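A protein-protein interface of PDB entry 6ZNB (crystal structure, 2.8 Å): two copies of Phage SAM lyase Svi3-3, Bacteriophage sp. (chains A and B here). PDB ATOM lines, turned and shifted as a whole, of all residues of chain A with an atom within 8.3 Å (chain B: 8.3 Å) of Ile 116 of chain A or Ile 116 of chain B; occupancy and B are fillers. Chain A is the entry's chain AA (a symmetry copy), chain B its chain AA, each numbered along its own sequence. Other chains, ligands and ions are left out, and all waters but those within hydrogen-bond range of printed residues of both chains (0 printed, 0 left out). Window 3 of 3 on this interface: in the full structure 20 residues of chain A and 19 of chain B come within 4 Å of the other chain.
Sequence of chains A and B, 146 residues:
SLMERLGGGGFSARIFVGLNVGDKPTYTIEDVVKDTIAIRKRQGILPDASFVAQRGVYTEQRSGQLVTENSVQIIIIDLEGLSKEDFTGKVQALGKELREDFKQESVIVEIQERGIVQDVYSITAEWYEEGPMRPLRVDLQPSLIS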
ATOM      1  N   GLY A   8     -29.070 -14.274  23.944  1.00  0.00           N
ATOM      2  CA  GLY A   8     -28.554 -15.383  24.719  1.00  0.00           C
ATOM      3  C   GLY A   8     -27.113 -15.751  24.459  1.00  0.00           C
ATOM      4  O   GLY A   8     -26.586 -16.652  25.119  1.00  0.00           O
ATOM      5  N   GLY A   9     -26.453 -15.083  23.517  1.00  0.00           N
ATOM      6  CA  GLY A   9     -25.068 -15.382  23.217  1.00  0.00           C
ATOM      7  C   GLY A   9     -24.589 -14.800  21.903  1.00  0.00           C
ATOM      8  O   GLY A   9     -24.110 -13.662  21.858  1.00  0.00           O
ATOM      9  N   GLY A  10     -24.711 -15.569  20.831  1.00  0.00           N
ATOM     10  CA  GLY A  10     -24.254 -15.158  19.519  1.00  0.00           C
ATOM     11  C   GLY A  10     -22.976 -15.879  19.123  1.00  0.00           C
ATOM     12  O   GLY A  10     -22.451 -16.728  19.845  1.00  0.00           O
ATOM     13  N   PHE A  11     -22.479 -15.514  17.945  1.00  0.00           N
ATOM     14  CA  PHE A  11     -21.274 -16.120  17.399  1.00  0.00           C
ATOM     15  C   PHE A  11     -20.045 -15.311  17.787  1.00  0.00           C
ATOM     16  O   PHE A  11     -20.047 -14.078  17.719  1.00  0.00           O
ATOM     17  CB  PHE A  11     -21.368 -16.231  15.876  1.00  0.00           C
ATOM     18  CG  PHE A  11     -22.431 -17.179  15.407  1.00  0.00           C
ATOM     19  CD1 PHE A  11     -22.207 -18.546  15.404  1.00  0.00           C
ATOM     20  CD2 PHE A  11     -23.658 -16.704  14.971  1.00  0.00           C
ATOM     21  CE1 PHE A  11     -23.187 -19.422  14.976  1.00  0.00           C
ATOM     22  CE2 PHE A  11     -24.641 -17.575  14.540  1.00  0.00           C
ATOM     23  CZ  PHE A  11     -24.405 -18.935  14.544  1.00  0.00           C
ATOM     24  N   SER A  12     -18.997 -16.014  18.204  1.00  0.00           N
ATOM     25  CA  SER A  12     -17.723 -15.396  18.531  1.00  0.00           C
ATOM     26  C   SER A  12     -16.600 -16.300  18.048  1.00  0.00           C
ATOM     27  O   SER A  12     -16.793 -17.497  17.820  1.00  0.00           O
ATOM     28  CB  SER A  12     -17.587 -15.129  20.038  1.00  0.00           C
ATOM     29  OG  SER A  12     -17.924 -16.278  20.797  1.00  0.00           O
ATOM     30  N   GLU A 110     -10.743 -20.665  16.255  1.00  0.00           N
ATOM     31  CA  GLU A 110     -11.761 -21.385  17.010  1.00  0.00           C
ATOM     32  C   GLU A 110     -13.049 -20.577  16.997  1.00  0.00           C
ATOM     33  O   GLU A 110     -13.090 -19.462  17.527  1.00  0.00           O
ATOM     34  CB  GLU A 110     -11.287 -21.645  18.444  1.00  0.00           C
ATOM     35  CG  GLU A 110     -12.384 -21.924  19.453  1.00  0.00           C
ATOM     36  CD  GLU A 110     -11.861 -21.905  20.877  1.00  0.00           C
ATOM     37  OE1 GLU A 110     -10.637 -22.079  21.062  1.00  0.00           O
ATOM     38  OE2 GLU A 110     -12.669 -21.709  21.810  1.00  0.00           O
ATOM     39  N   ILE A 111     -14.091 -21.133  16.386  1.00  0.00           N
ATOM     40  CA  ILE A 111     -15.392 -20.482  16.302  1.00  0.00           C
ATOM     41  C   ILE A 111     -16.265 -20.960  17.451  1.00  0.00           C
ATOM     42  O   ILE A 111     -16.327 -22.158  17.750  1.00  0.00           O
ATOM     43  CB  ILE A 111     -16.061 -20.760  14.943  1.00  0.00           C
ATOM     44  CG1 ILE A 111     -15.031 -20.687  13.809  1.00  0.00           C
ATOM     45  CG2 ILE A 111     -17.198 -19.778  14.699  1.00  0.00           C
ATOM     46  CD1 ILE A 111     -14.638 -19.279  13.424  1.00  0.00           C
ATOM     47  N   GLN A 112     -16.948 -20.019  18.096  1.00  0.00           N
ATOM     48  CA  GLN A 112     -17.825 -20.304  19.220  1.00  0.00           C
ATOM     49  C   GLN A 112     -19.219 -19.761  18.939  1.00  0.00           C
ATOM     50  O   GLN A 112     -19.401 -18.859  18.114  1.00  0.00           O
ATOM     51  CB  GLN A 112     -17.296 -19.677  20.517  1.00  0.00           C
ATOM     52  CG  GLN A 112     -15.892 -20.107  20.917  1.00  0.00           C
ATOM     53  CD  GLN A 112     -15.463 -19.510  22.248  1.00  0.00           C
ATOM     54  OE1 GLN A 112     -16.298 -19.199  23.100  1.00  0.00           O
ATOM     55  NE2 GLN A 112     -14.158 -19.349  22.432  1.00  0.00           N
ATOM     56  N   GLU A 113     -20.205 -20.325  19.633  1.00  0.00           N
ATOM     57  CA  GLU A 113     -21.559 -19.788  19.666  1.00  0.00           C
ATOM     58  C   GLU A 113     -22.070 -19.922  21.092  1.00  0.00           C
ATOM     59  O   GLU A 113     -22.168 -21.036  21.617  1.00  0.00           O
ATOM     60  CB  GLU A 113     -22.486 -20.511  18.685  1.00  0.00           C
ATOM     61  CG  GLU A 113     -23.785 -19.752  18.425  1.00  0.00           C
ATOM     62  CD  GLU A 113     -25.027 -20.623  18.489  1.00  0.00           C
ATOM     63  OE1 GLU A 113     -26.116 -20.069  18.756  1.00  0.00           O
ATOM     64  OE2 GLU A 113     -24.928 -21.843  18.250  1.00  0.00           O
ATOM     65  N   ARG A 114     -22.374 -18.786  21.718  1.00  0.00           N
ATOM     66  CA  ARG A 114     -22.761 -18.729  23.132  1.00  0.00           C
ATOM     67  C   ARG A 114     -21.683 -19.325  24.033  1.00  0.00           C
ATOM     68  O   ARG A 114     -21.977 -19.855  25.108  1.00  0.00           O
ATOM     69  CB  ARG A 114     -24.111 -19.414  23.377  1.00  0.00           C
ATOM     70  CG  ARG A 114     -25.128 -19.212  22.265  1.00  0.00           C
ATOM     71  CD  ARG A 114     -26.531 -19.040  22.825  1.00  0.00           C
ATOM     72  NE  ARG A 114     -26.840 -20.006  23.877  1.00  0.00           N
ATOM     73  CZ  ARG A 114     -27.217 -21.260  23.653  1.00  0.00           C
ATOM     74  NH1 ARG A 114     -27.332 -21.707  22.410  1.00  0.00           N
ATOM     75  NH2 ARG A 114     -27.479 -22.067  24.670  1.00  0.00           N
ATOM     76  N   GLY A 115     -20.424 -19.246  23.597  1.00  0.00           N
ATOM     77  CA  GLY A 115     -19.312 -19.787  24.344  1.00  0.00           C
ATOM     78  C   GLY A 115     -18.987 -21.232  24.049  1.00  0.00           C
ATOM     79  O   GLY A 115     -17.896 -21.689  24.413  1.00  0.00           O
ATOM     80  N   ILE A 116     -19.892 -21.965  23.407  1.00  0.00           N
ATOM     81  CA  ILE A 116     -19.646 -23.361  23.064  1.00  0.00           C
ATOM     82  C   ILE A 116     -18.856 -23.416  21.765  1.00  0.00           C
ATOM     83  O   ILE A 116     -19.217 -22.769  20.774  1.00  0.00           O
ATOM     84  CB  ILE A 116     -20.969 -24.131  22.944  1.00  0.00           C
ATOM     85  CG1 ILE A 116     -21.770 -24.014  24.241  1.00  0.00           C
ATOM     86  CG2 ILE A 116     -20.709 -25.591  22.604  1.00  0.00           C
ATOM     87  CD1 ILE A 116     -23.241 -24.309  24.076  1.00  0.00           C
ATOM     88  N   VAL A 117     -17.773 -24.189  21.765  1.00  0.00           N
ATOM     89  CA  VAL A 117     -16.909 -24.275  20.595  1.00  0.00           C
ATOM     90  C   VAL A 117     -17.630 -25.060  19.502  1.00  0.00           C
ATOM     91  O   VAL A 117     -18.045 -26.202  19.712  1.00  0.00           O
ATOM     92  CB  VAL A 117     -15.568 -24.927  20.953  1.00  0.00           C
ATOM     93  CG1 VAL A 117     -14.738 -25.131  19.703  1.00  0.00           C
ATOM     94  CG2 VAL A 117     -14.819 -24.072  21.964  1.00  0.00           C
ATOM     95  N   GLN A 118     -17.781 -24.438  18.332  1.00  0.00           N
ATOM     96  CA  GLN A 118     -18.406 -25.091  17.189  1.00  0.00           C
ATOM     97  C   GLN A 118     -17.370 -25.764  16.296  1.00  0.00           C
ATOM     98  O   GLN A 118     -17.508 -26.945  15.964  1.00  0.00           O
ATOM     99  CB  GLN A 118     -19.218 -24.075  16.383  1.00  0.00           C
ATOM    100  CG  GLN A 118     -20.273 -23.339  17.189  1.00  0.00           C
ATOM    101  CD  GLN A 118     -21.228 -24.282  17.893  1.00  0.00           C
ATOM    102  OE1 GLN A 118     -21.817 -25.167  17.271  1.00  0.00           O
ATOM    103  NE2 GLN A 118     -21.387 -24.098  19.199  1.00  0.00           N
ATOM    104  N   ASP A 119     -16.337 -25.024  15.895  1.00  0.00           N
ATOM    105  CA  ASP A 119     -15.253 -25.565  15.090  1.00  0.00           C
ATOM    106  C   ASP A 119     -13.934 -24.994  15.585  1.00  0.00           C
ATOM    107  O   ASP A 119     -13.889 -23.901  16.158  1.00  0.00           O
ATOM    108  CB  ASP A 119     -15.424 -25.238  13.599  1.00  0.00           C
ATOM    109  CG  ASP A 119     -16.873 -25.255  13.157  1.00  0.00           C
ATOM    110  OD1 ASP A 119     -17.446 -26.358  13.026  1.00  0.00           O
ATOM    111  OD2 ASP A 119     -17.440 -24.161  12.942  1.00  0.00           O
ATOM    112  N   GLY B  10     -21.678 -24.323  37.435  1.00  0.00           N
ATOM    113  CA  GLY B  10     -22.216 -23.236  38.229  1.00  0.00           C
ATOM    114  C   GLY B  10     -22.378 -21.971  37.403  1.00  0.00           C
ATOM    115  O   GLY B  10     -22.108 -21.932  36.202  1.00  0.00           O
ATOM    116  N   PHE B  11     -22.829 -20.922  38.084  1.00  0.00           N
ATOM    117  CA  PHE B  11     -23.067 -19.636  37.446  1.00  0.00           C
ATOM    118  C   PHE B  11     -21.835 -18.749  37.554  1.00  0.00           C
ATOM    119  O   PHE B  11     -21.206 -18.662  38.612  1.00  0.00           O
ATOM    120  CB  PHE B  11     -24.273 -18.936  38.073  1.00  0.00           C
ATOM    121  CG  PHE B  11     -25.573 -19.645  37.834  1.00  0.00           C
ATOM    122  CD1 PHE B  11     -26.237 -19.513  36.626  1.00  0.00           C
ATOM    123  CD2 PHE B  11     -26.130 -20.449  38.816  1.00  0.00           C
ATOM    124  CE1 PHE B  11     -27.433 -20.169  36.401  1.00  0.00           C
ATOM    125  CE2 PHE B  11     -27.326 -21.106  38.598  1.00  0.00           C
ATOM    126  CZ  PHE B  11     -27.977 -20.967  37.389  1.00  0.00           C
ATOM    127  N   SER B  12     -21.492 -18.099  36.446  1.00  0.00           N
ATOM    128  CA  SER B  12     -20.391 -17.151  36.409  1.00  0.00           C
ATOM    129  C   SER B  12     -20.781 -15.981  35.520  1.00  0.00           C
ATOM    130  O   SER B  12     -21.686 -16.081  34.687  1.00  0.00           O
ATOM    131  CB  SER B  12     -19.093 -17.800  35.905  1.00  0.00           C
ATOM    132  OG  SER B  12     -19.313 -18.531  34.710  1.00  0.00           O
ATOM    133  N   GLU B 110     -22.094 -10.239  30.842  1.00  0.00           N
ATOM    134  CA  GLU B 110     -22.359 -11.531  30.223  1.00  0.00           C
ATOM    135  C   GLU B 110     -22.450 -12.590  31.310  1.00  0.00           C
ATOM    136  O   GLU B 110     -21.467 -12.849  32.010  1.00  0.00           O
ATOM    137  CB  GLU B 110     -21.266 -11.877  29.205  1.00  0.00           C
ATOM    138  CG  GLU B 110     -21.137 -13.348  28.862  1.00  0.00           C
ATOM    139  CD  GLU B 110     -19.878 -13.635  28.066  1.00  0.00           C
ATOM    140  OE1 GLU B 110     -19.338 -12.691  27.449  1.00  0.00           O
ATOM    141  OE2 GLU B 110     -19.422 -14.798  28.062  1.00  0.00           O
ATOM    142  N   ILE B 111     -23.628 -13.190  31.454  1.00  0.00           N
ATOM    143  CA  ILE B 111     -23.862 -14.232  32.447  1.00  0.00           C
ATOM    144  C   ILE B 111     -23.649 -15.593  31.803  1.00  0.00           C
ATOM    145  O   ILE B 111     -24.118 -15.852  30.690  1.00  0.00           O
ATOM    146  CB  ILE B 111     -25.277 -14.115  33.044  1.00  0.00           C
ATOM    147  CG1 ILE B 111     -25.638 -12.646  33.293  1.00  0.00           C
ATOM    148  CG2 ILE B 111     -25.378 -14.918  34.333  1.00  0.00           C
ATOM    149  CD1 ILE B 111     -24.980 -12.048  34.516  1.00  0.00           C
ATOM    150  N   GLN B 112     -22.940 -16.468  32.511  1.00  0.00           N
ATOM    151  CA  GLN B 112     -22.641 -17.811  32.042  1.00  0.00           C
ATOM    152  C   GLN B 112     -23.116 -18.834  33.063  1.00  0.00           C
ATOM    153  O   GLN B 112     -23.292 -18.524  34.246  1.00  0.00           O
ATOM    154  CB  GLN B 112     -21.135 -18.000  31.807  1.00  0.00           C
ATOM    155  CG  GLN B 112     -20.507 -17.024  30.822  1.00  0.00           C
ATOM    156  CD  GLN B 112     -19.035 -17.317  30.580  1.00  0.00           C
ATOM    157  OE1 GLN B 112     -18.586 -18.457  30.716  1.00  0.00           O
ATOM    158  NE2 GLN B 112     -18.278 -16.289  30.216  1.00  0.00           N
ATOM    159  N   GLU B 113     -23.327 -20.061  32.591  1.00  0.00           N
ATOM    160  CA  GLU B 113     -23.562 -21.212  33.452  1.00  0.00           C
ATOM    161  C   GLU B 113     -22.809 -22.391  32.855  1.00  0.00           C
ATOM    162  O   GLU B 113     -23.082 -22.795  31.719  1.00  0.00           O
ATOM    163  CB  GLU B 113     -25.052 -21.531  33.589  1.00  0.00           C
ATOM    164  CG  GLU B 113     -25.355 -22.475  34.750  1.00  0.00           C
ATOM    165  CD  GLU B 113     -26.297 -23.609  34.390  1.00  0.00           C
ATOM    166  OE1 GLU B 113     -26.243 -24.654  35.075  1.00  0.00           O
ATOM    167  OE2 GLU B 113     -27.104 -23.455  33.451  1.00  0.00           O
ATOM    168  N   ARG B 114     -21.851 -22.924  33.613  1.00  0.00           N
ATOM    169  CA  ARG B 114     -20.951 -23.982  33.141  1.00  0.00           C
ATOM    170  C   ARG B 114     -20.184 -23.551  31.894  1.00  0.00           C
ATOM    171  O   ARG B 114     -19.816 -24.381  31.058  1.00  0.00           O
ATOM    172  CB  ARG B 114     -21.704 -25.294  32.887  1.00  0.00           C
ATOM    173  CG  ARG B 114     -22.817 -25.581  33.883  1.00  0.00           C
ATOM    174  CD  ARG B 114     -22.890 -27.063  34.217  1.00  0.00           C
ATOM    175  NE  ARG B 114     -22.785 -27.912  33.033  1.00  0.00           N
ATOM    176  CZ  ARG B 114     -23.794 -28.175  32.210  1.00  0.00           C
ATOM    177  NH1 ARG B 114     -24.991 -27.651  32.438  1.00  0.00           N
ATOM    178  NH2 ARG B 114     -23.608 -28.959  31.158  1.00  0.00           N
ATOM    179  N   GLY B 115     -19.941 -22.245  31.760  1.00  0.00           N
ATOM    180  CA  GLY B 115     -19.242 -21.704  30.617  1.00  0.00           C
ATOM    181  C   GLY B 115     -20.120 -21.338  29.444  1.00  0.00           C
ATOM    182  O   GLY B 115     -19.661 -20.612  28.553  1.00  0.00           O
ATOM    183  N   ILE B 116     -21.361 -21.813  29.412  1.00  0.00           N
ATOM    184  CA  ILE B 116     -22.280 -21.488  28.328  1.00  0.00           C
ATOM    185  C   ILE B 116     -22.931 -20.144  28.621  1.00  0.00           C
ATOM    186  O   ILE B 116     -23.441 -19.913  29.724  1.00  0.00           O
ATOM    187  CB  ILE B 116     -23.334 -22.592  28.160  1.00  0.00           C
ATOM    188  CG1 ILE B 116     -22.656 -23.941  27.923  1.00  0.00           C
ATOM    189  CG2 ILE B 116     -24.280 -22.258  27.016  1.00  0.00           C
ATOM    190  CD1 ILE B 116     -23.541 -25.127  28.218  1.00  0.00           C
ATOM    191  N   VAL B 117     -22.914 -19.252  27.634  1.00  0.00           N
ATOM    192  CA  VAL B 117     -23.457 -17.913  27.819  1.00  0.00           C
ATOM    193  C   VAL B 117     -24.980 -18.000  27.890  1.00  0.00           C
ATOM    194  O   VAL B 117     -25.628 -18.514  26.976  1.00  0.00           O
ATOM    195  CB  VAL B 117     -23.008 -16.979  26.690  1.00  0.00           C
ATOM    196  CG1 VAL B 117     -23.689 -15.633  26.824  1.00  0.00           C
ATOM    197  CG2 VAL B 117     -21.495 -16.822  26.705  1.00  0.00           C
ATOM    198  N   GLN B 118     -25.548 -17.498  28.987  1.00  0.00           N
ATOM    199  CA  GLN B 118     -26.996 -17.472  29.161  1.00  0.00           C
ATOM    200  C   GLN B 118     -27.591 -16.155  28.677  1.00  0.00           C
ATOM    201  O   GLN B 118     -28.541 -16.154  27.888  1.00  0.00           O
ATOM    202  CB  GLN B 118     -27.353 -17.706  30.630  1.00  0.00           C
ATOM    203  CG  GLN B 118     -26.793 -18.992  31.211  1.00  0.00           C
ATOM    204  CD  GLN B 118     -27.194 -20.214  30.409  1.00  0.00           C
ATOM    205  OE1 GLN B 118     -28.374 -20.436  30.141  1.00  0.00           O
ATOM    206  NE2 GLN B 118     -26.208 -21.015  30.020  1.00  0.00           N
ATOM    207  N   ASP B 119     -27.051 -15.032  29.148  1.00  0.00           N
ATOM    208  CA  ASP B 119     -27.490 -13.713  28.719  1.00  0.00           C
ATOM    209  C   ASP B 119     -26.275 -12.815  28.553  1.00  0.00           C
ATOM    210  O   ASP B 119     -25.238 -13.023  29.189  1.00  0.00           O
ATOM    211  CB  ASP B 119     -28.464 -13.075  29.723  1.00  0.00           C
ATOM    212  CG  ASP B 119     -29.387 -14.088  30.368  1.00  0.00           C
ATOM    213  OD1 ASP B 119     -30.325 -14.559  29.691  1.00  0.00           O
ATOM    214  OD2 ASP B 119     -29.172 -14.413  31.557  1.00  0.00           O
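The backbone NH of Val 117 of chain B is in hydrogen-bond range of the backbone carbonyl oxygen of Arg 114 of chain A (2.8 Å).
The backbone carbonyl oxygen of Gly 8 of chain A lies close to the backbone carbonyl oxygen of Val 117 of chain B.
The backbone carbonyl oxygen (O) of Gly 8 of chain A lies close to the backbone carbonyl oxygen (O) of Gln 118 of chain B (3.4 Å).
The backbone NH (N) of Gln 118 of chain B is in hydrogen-bond range of the backbone carbonyl oxygen (O) of Ile 111 of chain B (2.8 Å).
The side-chain amide nitrogen (NE2) of Gln 118 of chain B sits at hydrogen-bond distance from the backbone carbonyl oxygen (O) of Ile 116 of chain B, at 3.0 Å.
O of Gly 10 of chain A lies within hydrogen-bond range of N of Arg 114 of chain A.
NE2 of Gln 118 of chain A sits at hydrogen-bond distance from O of Ile 116 of chain A, 3.0 Å away.
Among the printed residues, pairs that only touch across the chains: Arg 114 of chain A with Ile 116 of chain B (3.6 Å), Ile 116 of chain A with Ile 116 of chain B (3.7 Å) and Gly 9 of chain A with Val 117 of chain B (3.9 Å).
Ile 116 of chain A touches one residue of chain B.
Of chain A, only Arg 114 and Ile 116 come within 4 Å of Ile 116 of chain B.
Printed residues of chain A within 4 Å of Gln 118 of chain B: Gly 8 (3.3 Å).
Printed residues of chain B within 4 Å of Gly 8 of chain A: Val 117 (2.8 Å) and Gln 118 (3.3 Å).
The nearest residue of chain B that does not touch Ile 116 of chain A is Gly 115 of chain B (5.3 Å).
Of the 15 printed residues of chain A, 4 touch a printed residue of chain B.
Hydrophobic or aromatic side chains of chain A within 4 Å of the printed part of chain B: Ile 116.
Along chain A the printed residues that touch a printed residue of chain B span positions 8 to 116.
Of the 13 printed residues of chain B, 3 touch a printed residue of chain A.
Hydrophobic or aromatic side chains of chain B that line the printed part of chain A: Ile 116 and Val 117.
Along chain B the printed residues that touch a printed residue of chain A span positions 116 to 118.
Among the printed residues, 6 pairs touch across the chains.
Among the printed residues, no Asp or Glu carboxylate lies within 4 Å of a Lys or Arg side-chain nitrogen of the other chain.
Arg 114 of chain A touches Ile 116 of chain B, but with the chains exchanged Ile 116 of chain A does not touch Arg 114 of chain B (7.1 Å).
Arg 114 of chain A touches Val 117 of chain B, but with the chains exchanged Val 117 of chain A does not touch Arg 114 of chain B (9.5 Å).
Ile 116 of chain A touches its own counterpart, Ile 116 of chain B.
Positions printed for both chains: 10, 11, 12, 110, 111, 112, 113, 114, 115, 116, 117, 118 and 119.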
